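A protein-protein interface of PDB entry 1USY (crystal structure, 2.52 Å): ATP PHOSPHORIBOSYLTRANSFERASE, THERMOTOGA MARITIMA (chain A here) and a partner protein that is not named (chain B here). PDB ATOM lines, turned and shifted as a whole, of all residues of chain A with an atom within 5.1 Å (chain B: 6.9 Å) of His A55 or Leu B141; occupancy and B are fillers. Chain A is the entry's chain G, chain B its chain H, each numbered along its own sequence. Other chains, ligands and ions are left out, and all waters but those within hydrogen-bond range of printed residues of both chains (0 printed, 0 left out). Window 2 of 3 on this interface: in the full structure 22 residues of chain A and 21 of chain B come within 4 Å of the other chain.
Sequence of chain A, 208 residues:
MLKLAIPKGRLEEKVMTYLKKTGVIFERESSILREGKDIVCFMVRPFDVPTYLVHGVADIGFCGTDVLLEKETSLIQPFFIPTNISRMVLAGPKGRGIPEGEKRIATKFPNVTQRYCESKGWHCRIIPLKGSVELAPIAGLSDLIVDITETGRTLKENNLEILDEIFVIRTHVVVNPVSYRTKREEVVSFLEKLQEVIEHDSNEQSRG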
ATOM      1  N   PRO A  50       4.638   2.990 -13.481  1.00  0.00           N
ATOM      2  CA  PRO A  50       4.203   2.386 -12.209  1.00  0.00           C
ATOM      3  C   PRO A  50       3.077   3.174 -11.558  1.00  0.00           C
ATOM      4  O   PRO A  50       2.205   2.563 -10.905  1.00  0.00           O
ATOM      5  CB  PRO A  50       5.449   2.415 -11.320  1.00  0.00           C
ATOM      6  CG  PRO A  50       6.529   3.047 -12.099  1.00  0.00           C
ATOM      7  CD  PRO A  50       6.083   3.289 -13.498  1.00  0.00           C
ATOM      8  N   THR A  51       3.046   4.495 -11.702  1.00  0.00           N
ATOM      9  CA  THR A  51       1.981   5.174 -10.966  1.00  0.00           C
ATOM     10  C   THR A  51       0.639   4.904 -11.606  1.00  0.00           C
ATOM     11  O   THR A  51      -0.344   4.826 -10.912  1.00  0.00           O
ATOM     12  CB  THR A  51       2.291   6.649 -10.590  1.00  0.00           C
ATOM     13  OG1 THR A  51       1.359   7.556 -11.192  1.00  0.00           O
ATOM     14  CG2 THR A  51       3.669   7.066 -11.111  1.00  0.00           C
ATOM     15  N   TYR A  52       0.627   4.649 -12.918  1.00  0.00           N
ATOM     16  CA  TYR A  52      -0.592   4.212 -13.638  1.00  0.00           C
ATOM     17  C   TYR A  52      -1.033   2.782 -13.274  1.00  0.00           C
ATOM     18  O   TYR A  52      -2.215   2.499 -13.118  1.00  0.00           O
ATOM     19  CB  TYR A  52      -0.390   4.328 -15.158  1.00  0.00           C
ATOM     20  CG  TYR A  52      -0.744   5.705 -15.739  1.00  0.00           C
ATOM     21  CD1 TYR A  52       0.168   6.761 -15.681  1.00  0.00           C
ATOM     22  CD2 TYR A  52      -1.996   5.948 -16.324  1.00  0.00           C
ATOM     23  CE1 TYR A  52      -0.139   8.025 -16.182  1.00  0.00           C
ATOM     24  CE2 TYR A  52      -2.328   7.223 -16.822  1.00  0.00           C
ATOM     25  CZ  TYR A  52      -1.388   8.252 -16.744  1.00  0.00           C
ATOM     26  OH  TYR A  52      -1.673   9.497 -17.243  1.00  0.00           O
ATOM     27  N   LEU A  53      -0.068   1.884 -13.145  1.00  0.00           N
ATOM     28  CA  LEU A  53      -0.340   0.495 -12.856  1.00  0.00           C
ATOM     29  C   LEU A  53      -0.697   0.276 -11.408  1.00  0.00           C
ATOM     30  O   LEU A  53      -1.633  -0.475 -11.108  1.00  0.00           O
ATOM     31  CB  LEU A  53       0.884  -0.323 -13.175  1.00  0.00           C
ATOM     32  CG  LEU A  53       0.742  -1.193 -14.414  1.00  0.00           C
ATOM     33  CD1 LEU A  53      -0.022  -0.497 -15.488  1.00  0.00           C
ATOM     34  CD2 LEU A  53       2.095  -1.468 -14.911  1.00  0.00           C
ATOM     35  N   VAL A  54       0.059   0.928 -10.515  1.00  0.00           N
ATOM     36  CA  VAL A  54      -0.044   0.703  -9.072  1.00  0.00           C
ATOM     37  C   VAL A  54      -1.418   1.107  -8.555  1.00  0.00           C
ATOM     38  O   VAL A  54      -1.956   0.475  -7.671  1.00  0.00           O
ATOM     39  CB  VAL A  54       1.147   1.391  -8.295  1.00  0.00           C
ATOM     40  CG1 VAL A  54       0.796   1.728  -6.851  1.00  0.00           C
ATOM     41  CG2 VAL A  54       2.406   0.508  -8.325  1.00  0.00           C
ATOM     42  N   HIS A  55      -2.012   2.135  -9.134  1.00  0.00           N
ATOM     43  CA  HIS A  55      -3.357   2.553  -8.733  1.00  0.00           C
ATOM     44  C   HIS A  55      -4.412   1.759  -9.534  1.00  0.00           C
ATOM     45  O   HIS A  55      -5.616   2.014  -9.429  1.00  0.00           O
ATOM     46  CB  HIS A  55      -3.572   4.081  -8.905  1.00  0.00           C
ATOM     47  CG  HIS A  55      -2.538   4.946  -8.234  1.00  0.00           C
ATOM     48  ND1 HIS A  55      -2.800   6.243  -7.844  1.00  0.00           N
ATOM     49  CD2 HIS A  55      -1.245   4.711  -7.899  1.00  0.00           C
ATOM     50  CE1 HIS A  55      -1.718   6.768  -7.297  1.00  0.00           C
ATOM     51  NE2 HIS A  55      -0.758   5.858  -7.322  1.00  0.00           N
ATOM     52  N   GLY A  56      -3.966   0.805 -10.338  1.00  0.00           N
ATOM     53  CA  GLY A  56      -4.879   0.056 -11.181  1.00  0.00           C
ATOM     54  C   GLY A  56      -5.733   0.922 -12.103  1.00  0.00           C
ATOM     55  O   GLY A  56      -6.944   0.687 -12.258  1.00  0.00           O
ATOM     56  N   VAL A  57      -5.115   1.940 -12.704  1.00  0.00           N
ATOM     57  CA  VAL A  57      -5.792   2.743 -13.729  1.00  0.00           C
ATOM     58  C   VAL A  57      -5.332   2.314 -15.113  1.00  0.00           C
ATOM     59  O   VAL A  57      -5.949   2.658 -16.096  1.00  0.00           O
ATOM     60  CB  VAL A  57      -5.635   4.242 -13.507  1.00  0.00           C
ATOM     61  CG1 VAL A  57      -5.894   4.569 -12.067  1.00  0.00           C
ATOM     62  CG2 VAL A  57      -4.285   4.722 -13.941  1.00  0.00           C
ATOM     63  N   ARG B 104      -8.152  15.271  -6.104  1.00  0.00           N
ATOM     64  CA  ARG B 104      -6.941  14.684  -6.671  1.00  0.00           C
ATOM     65  C   ARG B 104      -6.555  15.585  -7.840  1.00  0.00           C
ATOM     66  O   ARG B 104      -7.393  15.895  -8.681  1.00  0.00           O
ATOM     67  CB  ARG B 104      -7.126  13.227  -7.144  1.00  0.00           C
ATOM     68  CG  ARG B 104      -8.057  12.351  -6.339  1.00  0.00           C
ATOM     69  CD  ARG B 104      -7.852  10.849  -6.526  1.00  0.00           C
ATOM     70  NE  ARG B 104      -8.267  10.332  -7.835  1.00  0.00           N
ATOM     71  CZ  ARG B 104      -9.527  10.191  -8.265  1.00  0.00           C
ATOM     72  NH1 ARG B 104     -10.566  10.544  -7.509  1.00  0.00           N
ATOM     73  NH2 ARG B 104      -9.752   9.693  -9.478  1.00  0.00           N
ATOM     74  N   ILE B 105      -5.316  16.060  -7.854  1.00  0.00           N
ATOM     75  CA  ILE B 105      -4.862  16.944  -8.939  1.00  0.00           C
ATOM     76  C   ILE B 105      -3.515  16.459  -9.443  1.00  0.00           C
ATOM     77  O   ILE B 105      -2.568  16.343  -8.663  1.00  0.00           O
ATOM     78  CB  ILE B 105      -4.742  18.392  -8.468  1.00  0.00           C
ATOM     79  CG1 ILE B 105      -6.033  18.883  -7.816  1.00  0.00           C
ATOM     80  CG2 ILE B 105      -4.352  19.285  -9.626  1.00  0.00           C
ATOM     81  CD1 ILE B 105      -5.977  20.362  -7.370  1.00  0.00           C
ATOM     82  N   ALA B 106      -3.470  16.104 -10.727  1.00  0.00           N
ATOM     83  CA  ALA B 106      -2.256  15.681 -11.409  1.00  0.00           C
ATOM     84  C   ALA B 106      -1.620  16.894 -12.075  1.00  0.00           C
ATOM     85  O   ALA B 106      -2.329  17.757 -12.581  1.00  0.00           O
ATOM     86  CB  ALA B 106      -2.589  14.624 -12.456  1.00  0.00           C
ATOM     87  N   ARG B 125      -5.100  16.121  -2.971  1.00  0.00           N
ATOM     88  CA  ARG B 125      -4.078  15.106  -3.100  1.00  0.00           C
ATOM     89  C   ARG B 125      -3.396  15.288  -4.473  1.00  0.00           C
ATOM     90  O   ARG B 125      -4.051  15.261  -5.513  1.00  0.00           O
ATOM     91  CB  ARG B 125      -4.750  13.730  -2.887  1.00  0.00           C
ATOM     92  CG  ARG B 125      -4.025  12.482  -3.356  1.00  0.00           C
ATOM     93  CD  ARG B 125      -3.167  11.757  -2.313  1.00  0.00           C
ATOM     94  NE  ARG B 125      -1.790  11.700  -2.814  1.00  0.00           N
ATOM     95  CZ  ARG B 125      -1.404  11.072  -3.940  1.00  0.00           C
ATOM     96  NH1 ARG B 125      -2.290  10.385  -4.677  1.00  0.00           N
ATOM     97  NH2 ARG B 125      -0.124  11.119  -4.326  1.00  0.00           N
ATOM     98  N   ILE B 127      -0.682  14.520  -7.456  1.00  0.00           N
ATOM     99  CA  ILE B 127      -0.098  13.380  -8.128  1.00  0.00           C
ATOM    100  C   ILE B 127       0.907  13.920  -9.130  1.00  0.00           C
ATOM    101  O   ILE B 127       0.531  14.366 -10.194  1.00  0.00           O
ATOM    102  CB  ILE B 127      -1.244  12.570  -8.795  1.00  0.00           C
ATOM    103  CG1 ILE B 127      -2.220  12.104  -7.722  1.00  0.00           C
ATOM    104  CG2 ILE B 127      -0.714  11.350  -9.561  1.00  0.00           C
ATOM    105  CD1 ILE B 127      -3.507  11.664  -8.269  1.00  0.00           C
ATOM    106  N   LEU B 129       3.330  14.294 -12.162  1.00  0.00           N
ATOM    107  CA  LEU B 129       3.622  13.552 -13.411  1.00  0.00           C
ATOM    108  C   LEU B 129       4.747  14.199 -14.249  1.00  0.00           C
ATOM    109  O   LEU B 129       5.134  15.336 -14.029  1.00  0.00           O
ATOM    110  CB  LEU B 129       2.370  13.325 -14.281  1.00  0.00           C
ATOM    111  CG  LEU B 129       1.220  12.514 -13.689  1.00  0.00           C
ATOM    112  CD1 LEU B 129      -0.036  12.629 -14.545  1.00  0.00           C
ATOM    113  CD2 LEU B 129       1.594  11.050 -13.487  1.00  0.00           C
ATOM    114  N   LEU B 135      -4.193  13.178 -19.711  1.00  0.00           N
ATOM    115  CA  LEU B 135      -4.777  11.912 -19.296  1.00  0.00           C
ATOM    116  C   LEU B 135      -4.826  12.001 -17.784  1.00  0.00           C
ATOM    117  O   LEU B 135      -4.227  12.904 -17.186  1.00  0.00           O
ATOM    118  CB  LEU B 135      -3.941  10.715 -19.721  1.00  0.00           C
ATOM    119  CG  LEU B 135      -3.363  10.665 -21.138  1.00  0.00           C
ATOM    120  CD1 LEU B 135      -2.102   9.823 -21.134  1.00  0.00           C
ATOM    121  CD2 LEU B 135      -4.372  10.114 -22.155  1.00  0.00           C
ATOM    122  N   ALA B 136      -5.546  11.105 -17.137  1.00  0.00           N
ATOM    123  CA  ALA B 136      -5.541  11.112 -15.668  1.00  0.00           C
ATOM    124  C   ALA B 136      -6.949  11.346 -15.192  1.00  0.00           C
ATOM    125  O   ALA B 136      -7.469  10.481 -14.492  1.00  0.00           O
ATOM    126  CB  ALA B 136      -4.508  12.143 -15.041  1.00  0.00           C
ATOM    127  N   PRO B 137      -7.594  12.462 -15.559  1.00  0.00           N
ATOM    128  CA  PRO B 137      -9.059  12.527 -15.454  1.00  0.00           C
ATOM    129  C   PRO B 137      -9.729  11.280 -16.103  1.00  0.00           C
ATOM    130  O   PRO B 137     -10.424  10.497 -15.410  1.00  0.00           O
ATOM    131  CB  PRO B 137      -9.387  13.838 -16.159  1.00  0.00           C
ATOM    132  CG  PRO B 137      -8.170  14.702 -15.852  1.00  0.00           C
ATOM    133  CD  PRO B 137      -7.034  13.745 -16.036  1.00  0.00           C
ATOM    134  N   ILE B 138      -9.483  11.052 -17.386  1.00  0.00           N
ATOM    135  CA  ILE B 138      -9.751   9.729 -17.948  1.00  0.00           C
ATOM    136  C   ILE B 138      -8.577   8.870 -17.529  1.00  0.00           C
ATOM    137  O   ILE B 138      -7.415   9.255 -17.653  1.00  0.00           O
ATOM    138  CB  ILE B 138      -9.807   9.785 -19.449  1.00  0.00           C
ATOM    139  CG1 ILE B 138      -9.568  11.235 -19.906  1.00  0.00           C
ATOM    140  CG2 ILE B 138     -11.135   9.212 -19.939  1.00  0.00           C
ATOM    141  CD1 ILE B 138      -8.155  11.552 -20.312  1.00  0.00           C
ATOM    142  N   ALA B 139      -8.885   7.702 -17.026  1.00  0.00           N
ATOM    143  CA  ALA B 139      -7.916   6.862 -16.379  1.00  0.00           C
ATOM    144  C   ALA B 139      -8.340   6.875 -14.950  1.00  0.00           C
ATOM    145  O   ALA B 139      -8.284   5.857 -14.276  1.00  0.00           O
ATOM    146  CB  ALA B 139      -6.520   7.427 -16.529  1.00  0.00           C
ATOM    147  N   GLY B 140      -8.783   8.045 -14.500  1.00  0.00           N
ATOM    148  CA  GLY B 140      -9.169   8.245 -13.125  1.00  0.00           C
ATOM    149  C   GLY B 140      -8.006   8.266 -12.159  1.00  0.00           C
ATOM    150  O   GLY B 140      -8.206   7.917 -11.006  1.00  0.00           O
ATOM    151  N   LEU B 141      -6.823   8.658 -12.617  1.00  0.00           N
ATOM    152  CA  LEU B 141      -5.701   8.970 -11.756  1.00  0.00           C
ATOM    153  C   LEU B 141      -6.004  10.232 -10.973  1.00  0.00           C
ATOM    154  O   LEU B 141      -5.578  10.366  -9.851  1.00  0.00           O
ATOM    155  CB  LEU B 141      -4.468   9.277 -12.604  1.00  0.00           C
ATOM    156  CG  LEU B 141      -3.330   8.291 -12.758  1.00  0.00           C
ATOM    157  CD1 LEU B 141      -2.170   9.037 -13.367  1.00  0.00           C
ATOM    158  CD2 LEU B 141      -2.891   7.657 -11.429  1.00  0.00           C
ATOM    159  N   SER B 142      -6.691  11.185 -11.582  1.00  0.00           N
ATOM    160  CA  SER B 142      -6.896  12.491 -10.965  1.00  0.00           C
ATOM    161  C   SER B 142      -8.340  12.925 -11.261  1.00  0.00           C
ATOM    162  O   SER B 142      -9.036  12.267 -12.037  1.00  0.00           O
ATOM    163  CB  SER B 142      -5.850  13.474 -11.501  1.00  0.00           C
ATOM    164  OG  SER B 142      -6.411  14.527 -12.252  1.00  0.00           O
ATOM    165  N   ASP B 143      -8.814  13.992 -10.624  1.00  0.00           N
ATOM    166  CA  ASP B 143     -10.132  14.539 -10.935  1.00  0.00           C
ATOM    167  C   ASP B 143      -9.922  15.770 -11.764  1.00  0.00           C
ATOM    168  O   ASP B 143     -10.818  16.201 -12.507  1.00  0.00           O
ATOM    169  CB  ASP B 143     -10.870  14.945  -9.661  1.00  0.00           C
ATOM    170  CG  ASP B 143     -11.182  13.760  -8.747  1.00  0.00           C
ATOM    171  OD1 ASP B 143     -12.062  12.915  -9.110  1.00  0.00           O
ATOM    172  OD2 ASP B 143     -10.597  13.616  -7.635  1.00  0.00           O
ATOM    173  N   LEU B 144      -8.705  16.304 -11.640  1.00  0.00           N
ATOM    174  CA  LEU B 144      -8.382  17.672 -11.988  1.00  0.00           C
ATOM    175  C   LEU B 144      -6.918  17.721 -12.335  1.00  0.00           C
ATOM    176  O   LEU B 144      -6.140  16.946 -11.802  1.00  0.00           O
ATOM    177  CB  LEU B 144      -8.531  18.509 -10.737  1.00  0.00           C
ATOM    178  CG  LEU B 144      -9.602  19.574 -10.583  1.00  0.00           C
ATOM    179  CD1 LEU B 144     -10.952  18.967 -10.833  1.00  0.00           C
ATOM    180  CD2 LEU B 144      -9.488  20.204  -9.180  1.00  0.00           C
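The backbone carbonyl oxygen of Ala B136 lies within hydrogen-bond range of the backbone NH of Leu B141 (2.7 Å).
The backbone NH (N) of Val A57 sits at hydrogen-bond distance from the backbone carbonyl oxygen (O) of Tyr A52 (3.0 Å).
O of Leu B141 sits at hydrogen-bond distance from NE of Arg B104.
Of the 8 printed residues of chain A, 4 touch a printed residue of chain B.
Printed residues of chain A that touch a printed residue of chain B: Thr A51, Tyr A52, His A55 and Val A57.
Printed residues of chain B that touch a printed residue of chain A: Leu B135, Ala B139 and Leu B141.
Along chain B the printed residues that touch a printed residue of chain A span positions 135 to 141.
Among the printed residues, no Asp or Glu carboxylate lies within 4 Å of a Lys or Arg side-chain nitrogen of the other chain.
His A55 touches just one residue of chain B: Leu B141.
Leu B141 touches just these residues of chain A: Thr A51, Tyr A52, His A55 and Val A57.
Printed residues of chain B within 4 Å of Val A57: Ala B139 and Leu B141.
Printed residues of chain B within 4 Å of Thr A51: Leu B141.
Of the printed residues of chain B, Tyr A52 touches Leu B135 (3.6 Å) and Leu B141 (3.6 Å).
Of the printed residues of chain A, Leu B135 touches Tyr A52 (3.6 Å).
Ala B136 touches none of the printed residues of chain A.
Ile B138 touches none of the printed residues of chain A.
The nearest residue of chain B that does not touch His A55 is Arg B125 (4.5 Å).
The nearest printed residue of chain A that does not touch Leu B141 is Leu A53 (6.7 Å).
The nearest printed residue of chain A that does not touch Leu B135 is Val A57 (8.2 Å).
Among the printed residues, merely in contact across the chains: Val A57 with Ala B139 (3.2 Å), Tyr A52 with Leu B141 (3.6 Å), Tyr A52 with Leu B135 (3.6 Å), Thr A51 with Leu B141 (3.8 Å), His A55 with Leu B141 (3.9 Å) and Val A57 with Leu B141 (3.9 Å).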
